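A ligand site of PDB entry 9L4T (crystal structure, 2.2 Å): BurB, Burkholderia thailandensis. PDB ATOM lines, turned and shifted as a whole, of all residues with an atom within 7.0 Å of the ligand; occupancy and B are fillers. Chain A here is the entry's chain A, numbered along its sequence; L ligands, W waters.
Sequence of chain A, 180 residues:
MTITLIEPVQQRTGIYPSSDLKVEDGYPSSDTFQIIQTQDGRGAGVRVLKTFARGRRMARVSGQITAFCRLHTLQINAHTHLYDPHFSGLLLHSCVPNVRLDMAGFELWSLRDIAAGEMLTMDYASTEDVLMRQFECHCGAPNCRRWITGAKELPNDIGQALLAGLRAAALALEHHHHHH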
ATOM      1  N   CYS A  69     -10.947  12.954   3.822  1.00  0.00           N
ATOM      2  CA  CYS A  69      -9.988  14.029   3.631  1.00  0.00           C
ATOM      3  C   CYS A  69      -9.239  13.812   2.323  1.00  0.00           C
ATOM      4  O   CYS A  69      -8.969  12.676   1.919  1.00  0.00           O
ATOM      5  CB  CYS A  69      -9.028  14.071   4.823  1.00  0.00           C
ATOM      6  SG  CYS A  69      -7.904  15.477   4.750  1.00  0.00           S
ATOM      7  N   ARG A  70      -8.908  14.911   1.649  1.00  0.00           N
ATOM      8  CA  ARG A  70      -8.369  14.856   0.297  1.00  0.00           C
ATOM      9  C   ARG A  70      -7.742  16.202  -0.011  1.00  0.00           C
ATOM     10  O   ARG A  70      -7.920  17.177   0.732  1.00  0.00           O
ATOM     11  CB  ARG A  70      -9.469  14.571  -0.735  1.00  0.00           C
ATOM     12  CG  ARG A  70      -9.526  13.181  -1.246  1.00  0.00           C
ATOM     13  CD  ARG A  70     -10.135  13.217  -2.627  1.00  0.00           C
ATOM     14  NE  ARG A  70     -11.560  13.527  -2.600  1.00  0.00           N
ATOM     15  CZ  ARG A  70     -12.246  14.004  -3.628  1.00  0.00           C
ATOM     16  NH1 ARG A  70     -11.651  14.336  -4.764  1.00  0.00           N
ATOM     17  NH2 ARG A  70     -13.568  14.147  -3.521  1.00  0.00           N
ATOM     18  N   LEU A  71      -7.021  16.272  -1.125  1.00  0.00           N
ATOM     19  CA  LEU A  71      -6.664  17.569  -1.674  1.00  0.00           C
ATOM     20  C   LEU A  71      -7.933  18.360  -1.948  1.00  0.00           C
ATOM     21  O   LEU A  71      -8.909  17.802  -2.470  1.00  0.00           O
ATOM     22  CB  LEU A  71      -5.851  17.416  -2.959  1.00  0.00           C
ATOM     23  CG  LEU A  71      -4.333  17.620  -2.790  1.00  0.00           C
ATOM     24  CD1 LEU A  71      -3.578  16.956  -3.938  1.00  0.00           C
ATOM     25  CD2 LEU A  71      -4.020  19.122  -2.707  1.00  0.00           C
ATOM     26  N   HIS A  72      -7.937  19.636  -1.564  1.00  0.00           N
ATOM     27  CA  HIS A  72      -9.071  20.549  -1.754  1.00  0.00           C
ATOM     28  C   HIS A  72     -10.293  20.217  -0.888  1.00  0.00           C
ATOM     29  O   HIS A  72     -11.381  20.720  -1.160  1.00  0.00           O
ATOM     30  CB  HIS A  72      -9.508  20.616  -3.231  1.00  0.00           C
ATOM     31  CG  HIS A  72      -8.390  20.867  -4.201  1.00  0.00           C
ATOM     32  ND1 HIS A  72      -8.379  20.337  -5.473  1.00  0.00           N
ATOM     33  CD2 HIS A  72      -7.262  21.603  -4.087  1.00  0.00           C
ATOM     34  CE1 HIS A  72      -7.275  20.715  -6.099  1.00  0.00           C
ATOM     35  NE2 HIS A  72      -6.585  21.488  -5.286  1.00  0.00           N
ATOM     36  N   THR A  73     -10.163  19.411   0.166  1.00  0.00           N
ATOM     37  CA  THR A  73     -11.249  19.297   1.137  1.00  0.00           C
ATOM     38  C   THR A  73     -10.895  20.097   2.380  1.00  0.00           C
ATOM     39  O   THR A  73      -9.729  20.166   2.783  1.00  0.00           O
ATOM     40  CB  THR A  73     -11.522  17.857   1.563  1.00  0.00           C
ATOM     41  OG1 THR A  73     -10.376  17.329   2.249  1.00  0.00           O
ATOM     42  CG2 THR A  73     -11.886  16.996   0.387  1.00  0.00           C
ATOM     43  N   LEU A  74     -11.918  20.696   2.976  1.00  0.00           N
ATOM     44  CA  LEU A  74     -11.818  21.307   4.288  1.00  0.00           C
ATOM     45  C   LEU A  74     -12.698  20.520   5.241  1.00  0.00           C
ATOM     46  O   LEU A  74     -13.752  20.026   4.845  1.00  0.00           O
ATOM     47  CB  LEU A  74     -12.220  22.772   4.213  1.00  0.00           C
ATOM     48  CG  LEU A  74     -11.132  23.423   3.356  1.00  0.00           C
ATOM     49  CD1 LEU A  74     -11.736  24.119   2.185  1.00  0.00           C
ATOM     50  CD2 LEU A  74     -10.294  24.346   4.186  1.00  0.00           C
ATOM     51  N   GLN A  75     -12.242  20.383   6.492  1.00  0.00           N
ATOM     52  CA  GLN A  75     -12.903  19.521   7.474  1.00  0.00           C
ATOM     53  C   GLN A  75     -14.124  20.210   8.060  1.00  0.00           C
ATOM     54  O   GLN A  75     -14.052  21.368   8.472  1.00  0.00           O
ATOM     55  CB  GLN A  75     -11.906  19.170   8.583  1.00  0.00           C
ATOM     56  CG  GLN A  75     -12.437  18.178   9.616  1.00  0.00           C
ATOM     57  CD  GLN A  75     -11.320  17.592  10.437  1.00  0.00           C
ATOM     58  OE1 GLN A  75     -10.140  17.798  10.138  1.00  0.00           O
ATOM     59  NE2 GLN A  75     -11.673  16.828  11.475  1.00  0.00           N
ATOM     60  N   HIS A  81     -16.058  16.052   5.505  1.00  0.00           N
ATOM     61  CA  HIS A  81     -15.197  17.033   4.886  1.00  0.00           C
ATOM     62  C   HIS A  81     -15.963  17.654   3.737  1.00  0.00           C
ATOM     63  O   HIS A  81     -16.894  17.063   3.179  1.00  0.00           O
ATOM     64  CB  HIS A  81     -13.888  16.393   4.413  1.00  0.00           C
ATOM     65  CG  HIS A  81     -13.104  15.769   5.530  1.00  0.00           C
ATOM     66  ND1 HIS A  81     -13.273  14.450   5.911  1.00  0.00           N
ATOM     67  CD2 HIS A  81     -12.165  16.285   6.366  1.00  0.00           C
ATOM     68  CE1 HIS A  81     -12.465  14.177   6.924  1.00  0.00           C
ATOM     69  NE2 HIS A  81     -11.782  15.272   7.217  1.00  0.00           N
ATOM     70  N   ASP A  84     -14.126  21.178  -2.093  1.00  0.00           N
ATOM     71  CA  ASP A  84     -14.307  22.441  -2.803  1.00  0.00           C
ATOM     72  C   ASP A  84     -13.060  22.733  -3.632  1.00  0.00           C
ATOM     73  O   ASP A  84     -12.184  23.505  -3.223  1.00  0.00           O
ATOM     74  CB  ASP A  84     -14.606  23.578  -1.827  1.00  0.00           C
ATOM     75  CG  ASP A  84     -14.760  24.904  -2.528  1.00  0.00           C
ATOM     76  OD1 ASP A  84     -14.700  24.924  -3.777  1.00  0.00           O
ATOM     77  OD2 ASP A  84     -14.971  25.926  -1.846  1.00  0.00           O
ATOM     78  N   SER A  88     -12.594  27.529  -1.917  1.00  0.00           N
ATOM     79  CA  SER A  88     -11.928  27.595  -0.620  1.00  0.00           C
ATOM     80  C   SER A  88     -10.787  26.576  -0.500  1.00  0.00           C
ATOM     81  O   SER A  88      -9.827  26.829   0.223  1.00  0.00           O
ATOM     82  CB  SER A  88     -12.946  27.390   0.495  1.00  0.00           C
ATOM     83  OG  SER A  88     -13.499  26.082   0.444  1.00  0.00           O
ATOM     84  N   GLY A  89     -10.894  25.429  -1.163  1.00  0.00           N
ATOM     85  CA  GLY A  89      -9.824  24.465  -1.183  1.00  0.00           C
ATOM     86  C   GLY A  89      -8.622  24.893  -2.004  1.00  0.00           C
ATOM     87  O   GLY A  89      -7.619  24.169  -2.057  1.00  0.00           O
ATOM     88  N   LEU A  90      -8.697  26.048  -2.658  1.00  0.00           N
ATOM     89  CA  LEU A  90      -7.603  26.601  -3.419  1.00  0.00           C
ATOM     90  C   LEU A  90      -6.780  27.607  -2.637  1.00  0.00           C
ATOM     91  O   LEU A  90      -5.799  28.149  -3.175  1.00  0.00           O
ATOM     92  CB  LEU A  90      -8.137  27.240  -4.703  1.00  0.00           C
ATOM     93  CG  LEU A  90      -8.889  26.260  -5.607  1.00  0.00           C
ATOM     94  CD1 LEU A  90      -9.441  26.950  -6.841  1.00  0.00           C
ATOM     95  CD2 LEU A  90      -7.971  25.135  -6.011  1.00  0.00           C
ATOM     96  N   LEU A  91      -7.139  27.898  -1.381  1.00  0.00           N
ATOM     97  CA  LEU A  91      -6.421  28.920  -0.633  1.00  0.00           C
ATOM     98  C   LEU A  91      -5.115  28.339  -0.137  1.00  0.00           C
ATOM     99  O   LEU A  91      -5.076  27.253   0.450  1.00  0.00           O
ATOM    100  CB  LEU A  91      -7.238  29.441   0.545  1.00  0.00           C
ATOM    101  CG  LEU A  91      -8.608  30.011   0.173  1.00  0.00           C
ATOM    102  CD1 LEU A  91      -9.479  30.128   1.430  1.00  0.00           C
ATOM    103  CD2 LEU A  91      -8.506  31.354  -0.544  1.00  0.00           C
ATOM    104  N   LEU A  92      -4.026  29.092  -0.382  1.00  0.00           N
ATOM    105  CA  LEU A  92      -2.736  28.691   0.138  1.00  0.00           C
ATOM    106  C   LEU A  92      -2.677  28.946   1.636  1.00  0.00           C
ATOM    107  O   LEU A  92      -3.446  29.747   2.206  1.00  0.00           O
ATOM    108  CB  LEU A  92      -1.615  29.438  -0.606  1.00  0.00           C
ATOM    109  CG  LEU A  92      -1.651  29.208  -2.127  1.00  0.00           C
ATOM    110  CD1 LEU A  92      -0.573  29.986  -2.884  1.00  0.00           C
ATOM    111  CD2 LEU A  92      -1.541  27.708  -2.433  1.00  0.00           C
ATOM    112  N   HIS A  93      -1.775  28.231   2.300  1.00  0.00           N
ATOM    113  CA  HIS A  93      -1.585  28.374   3.721  1.00  0.00           C
ATOM    114  C   HIS A  93      -0.717  29.586   4.070  1.00  0.00           C
ATOM    115  O   HIS A  93       0.143  30.005   3.286  1.00  0.00           O
ATOM    116  CB  HIS A  93      -0.927  27.116   4.298  1.00  0.00           C
ATOM    117  CG  HIS A  93      -0.340  27.313   5.660  1.00  0.00           C
ATOM    118  ND1 HIS A  93      -1.087  27.217   6.812  1.00  0.00           N
ATOM    119  CD2 HIS A  93       0.917  27.661   6.049  1.00  0.00           C
ATOM    120  CE1 HIS A  93      -0.316  27.465   7.859  1.00  0.00           C
ATOM    121  NE2 HIS A  93       0.902  27.746   7.414  1.00  0.00           N
ATOM    122  N   MET A 122      -4.945  31.140   4.494  1.00  0.00           N
ATOM    123  CA  MET A 122      -5.545  30.670   5.735  1.00  0.00           C
ATOM    124  C   MET A 122      -4.541  29.785   6.458  1.00  0.00           C
ATOM    125  O   MET A 122      -3.639  29.217   5.856  1.00  0.00           O
ATOM    126  CB  MET A 122      -6.876  29.929   5.445  1.00  0.00           C
ATOM    127  CG  MET A 122      -6.743  28.661   4.588  1.00  0.00           C
ATOM    128  SD  MET A 122      -8.344  27.839   4.141  1.00  0.00           S
ATOM    129  CE  MET A 122      -7.766  26.652   2.934  1.00  0.00           C
ATOM    130  N   TYR A 124      -3.976  26.455   7.633  1.00  0.00           N
ATOM    131  CA  TYR A 124      -4.531  25.126   7.422  1.00  0.00           C
ATOM    132  C   TYR A 124      -4.808  24.424   8.745  1.00  0.00           C
ATOM    133  O   TYR A 124      -5.796  23.692   8.866  1.00  0.00           O
ATOM    134  CB  TYR A 124      -3.582  24.279   6.566  1.00  0.00           C
ATOM    135  CG  TYR A 124      -3.580  24.627   5.075  1.00  0.00           C
ATOM    136  CD1 TYR A 124      -4.256  25.750   4.609  1.00  0.00           C
ATOM    137  CD2 TYR A 124      -2.907  23.841   4.141  1.00  0.00           C
ATOM    138  CE1 TYR A 124      -4.257  26.080   3.260  1.00  0.00           C
ATOM    139  CE2 TYR A 124      -2.894  24.167   2.773  1.00  0.00           C
ATOM    140  CZ  TYR A 124      -3.578  25.288   2.349  1.00  0.00           C
ATOM    141  OH  TYR A 124      -3.587  25.637   1.022  1.00  0.00           O
ATOM    142  N   THR A 127      -8.415  24.598  10.768  1.00  0.00           N
ATOM    143  CA  THR A 127      -9.576  23.782  10.426  1.00  0.00           C
ATOM    144  C   THR A 127      -9.267  22.295  10.295  1.00  0.00           C
ATOM    145  O   THR A 127     -10.163  21.473  10.521  1.00  0.00           O
ATOM    146  CB  THR A 127     -10.264  24.242   9.115  1.00  0.00           C
ATOM    147  OG1 THR A 127      -9.355  24.170   8.013  1.00  0.00           O
ATOM    148  CG2 THR A 127     -10.816  25.648   9.232  1.00  0.00           C
ATOM    149  N   GLU A 128      -8.028  21.924   9.949  1.00  0.00           N
ATOM    150  CA  GLU A 128      -7.716  20.556   9.552  1.00  0.00           C
ATOM    151  C   GLU A 128      -7.042  19.783  10.667  1.00  0.00           C
ATOM    152  O   GLU A 128      -6.035  20.233  11.238  1.00  0.00           O
ATOM    153  CB  GLU A 128      -6.828  20.569   8.306  1.00  0.00           C
ATOM    154  CG  GLU A 128      -7.408  21.396   7.119  1.00  0.00           C
ATOM    155  CD  GLU A 128      -8.872  21.030   6.791  1.00  0.00           C
ATOM    156  OE1 GLU A 128      -9.106  19.876   6.371  1.00  0.00           O
ATOM    157  OE2 GLU A 128      -9.779  21.890   6.943  1.00  0.00           O
ATOM    158  N   VAL A 130      -5.669  16.737   9.979  1.00  0.00           N
ATOM    159  CA  VAL A 130      -4.529  16.146   9.290  1.00  0.00           C
ATOM    160  C   VAL A 130      -4.610  16.657   7.866  1.00  0.00           C
ATOM    161  O   VAL A 130      -5.666  17.064   7.384  1.00  0.00           O
ATOM    162  CB  VAL A 130      -4.511  14.594   9.309  1.00  0.00           C
ATOM    163  CG1 VAL A 130      -4.544  14.047  10.738  1.00  0.00           C
ATOM    164  CG2 VAL A 130      -5.665  14.041   8.509  1.00  0.00           C
ATOM    165  N   LEU A 131      -3.454  16.666   7.211  1.00  0.00           N
ATOM    166  CA  LEU A 131      -3.325  17.110   5.829  1.00  0.00           C
ATOM    167  C   LEU A 131      -3.039  15.911   4.934  1.00  0.00           C
ATOM    168  O   LEU A 131      -2.384  14.948   5.348  1.00  0.00           O
ATOM    169  CB  LEU A 131      -2.207  18.144   5.687  1.00  0.00           C
ATOM    170  CG  LEU A 131      -2.363  19.495   6.379  1.00  0.00           C
ATOM    171  CD1 LEU A 131      -1.095  20.301   6.172  1.00  0.00           C
ATOM    172  CD2 LEU A 131      -3.589  20.253   5.866  1.00  0.00           C
ATOM    173  N   MET A 132      -3.550  15.979   3.703  1.00  0.00           N
ATOM    174  CA  MET A 132      -3.190  14.986   2.698  1.00  0.00           C
ATOM    175  C   MET A 132      -1.680  14.918   2.494  1.00  0.00           C
ATOM    176  O   MET A 132      -1.136  13.840   2.217  1.00  0.00           O
ATOM    177  CB  MET A 132      -3.908  15.321   1.381  1.00  0.00           C
ATOM    178  CG  MET A 132      -4.392  14.166   0.495  1.00  0.00           C
ATOM    179  SD  MET A 132      -4.940  12.621   1.259  1.00  0.00           S
ATOM    180  CE  MET A 132      -5.999  13.121   2.627  1.00  0.00           C
ATOM    181  N   ARG A 133      -0.985  16.049   2.668  1.00  0.00           N
ATOM    182  CA  ARG A 133       0.468  16.080   2.553  1.00  0.00           C
ATOM    183  C   ARG A 133       1.012  17.201   3.420  1.00  0.00           C
ATOM    184  O   ARG A 133       0.446  18.299   3.434  1.00  0.00           O
ATOM    185  CB  ARG A 133       0.889  16.277   1.095  1.00  0.00           C
ATOM    186  CG  ARG A 133       2.396  16.325   0.884  1.00  0.00           C
ATOM    187  CD  ARG A 133       2.860  15.210  -0.059  1.00  0.00           C
ATOM    188  NE  ARG A 133       2.491  15.475  -1.445  1.00  0.00           N
ATOM    189  CZ  ARG A 133       3.352  15.768  -2.411  1.00  0.00           C
ATOM    190  NH1 ARG A 133       4.656  15.843  -2.183  1.00  0.00           N
ATOM    191  NH2 ARG A 133       2.900  15.990  -3.650  1.00  0.00           N
ATOM    192  N   PHE A 135       4.258  19.831   4.205  1.00  0.00           N
ATOM    193  CA  PHE A 135       5.074  20.615   3.277  1.00  0.00           C
ATOM    194  C   PHE A 135       5.753  21.754   4.025  1.00  0.00           C
ATOM    195  O   PHE A 135       5.270  22.227   5.061  1.00  0.00           O
ATOM    196  CB  PHE A 135       4.209  21.175   2.134  1.00  0.00           C
ATOM    197  CG  PHE A 135       3.081  22.044   2.598  1.00  0.00           C
ATOM    198  CD1 PHE A 135       1.839  21.495   2.920  1.00  0.00           C
ATOM    199  CD2 PHE A 135       3.241  23.430   2.702  1.00  0.00           C
ATOM    200  CE1 PHE A 135       0.775  22.307   3.335  1.00  0.00           C
ATOM    201  CE2 PHE A 135       2.189  24.249   3.120  1.00  0.00           C
ATOM    202  CZ  PHE A 135       0.947  23.688   3.435  1.00  0.00           C
HETATM  203  N1  LIG L   1      -7.384  18.928   2.733  1.00  0.00           N
HETATM  204  C1  LIG L   1      -6.350  19.808   2.191  1.00  0.00           C
HETATM  205  C2  LIG L   1      -5.066  19.012   1.962  1.00  0.00           C
HETATM  206  O1  LIG L   1      -4.225  19.382   1.135  1.00  0.00           O
HETATM  207  C3  LIG L   1      -6.059  20.977   3.142  1.00  0.00           C
HETATM  208  C4  LIG L   1      -6.936  22.229   3.015  1.00  0.00           C
HETATM  209  S1  LIG L   1      -7.527  22.613   1.342  1.00  0.00           S
HETATM  210  C5  LIG L   1      -6.454  23.979   0.853  1.00  0.00           C
HETATM  211  O2  LIG L   1      -4.821  17.998   2.635  1.00  0.00           O
HETATM  212  O   HOH W   1      -7.004  18.369   5.594  1.00  0.00           O
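O2 of the ligand is in hydrogen-bond range of N of Met 132 (2.6 Å).
The backbone carbonyl oxygen of Thr 73 lies within hydrogen-bond range of a nitrogen (N1) of the ligand, at 2.7 Å.
The side-chain hydroxyl (OG1) of Thr 73 lies within hydrogen-bond range of a nitrogen (N1) of the ligand (3.4 Å).
The backbone carbonyl oxygen (O) of Arg 70 sits at hydrogen-bond distance from a nitrogen (N1) of the ligand (2.7 Å).
The side-chain hydroxyl (OG1) of Thr 73 is in hydrogen-bond range of the backbone carbonyl oxygen (O) of Arg 70 (2.9 Å).
The backbone NH (N) of Gly 89 lies within hydrogen-bond range of the backbone carbonyl oxygen (O) of Asp 84 (3.1 Å).
N of Tyr 124 lies within hydrogen-bond range of ND1 of His 93 (3.1 Å).
The backbone carbonyl oxygen of Leu 92 lies within hydrogen-bond range of the backbone NH of Met 122, at 3.1 Å.
A ring nitrogen (ND1) of His 93 lies close to the backbone carbonyl oxygen (O) of Met 122 (3.4 Å).
A sulfur (S1) of the ligand sits close to the backbone carbonyl oxygen of Gly 89, at 3.7 Å.
Merely in contact with the ligand: Leu 71 (3.9 Å), Leu 91 (3.6 Å), Met 122 (3.6 Å), Tyr 124 (3.3 Å) and Leu 131 (3.6 Å).
Hydrophobic or aromatic side chains that line the ligand: Leu 71, Met 122, Tyr 124, Leu 131 and Met 132.
Within 4 Å of the ligand: Arg 70, Leu 71, Thr 73, Gly 89, Leu 91, Met 122, Tyr 124, Leu 131 and Met 132.
Water W1 lies within hydrogen-bond range of O of Val 130 (2.6 Å), OE1 of Glu 128 (2.7 Å), N1 of the ligand (2.9 Å) and SG of Cys 69 (3.1 Å).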
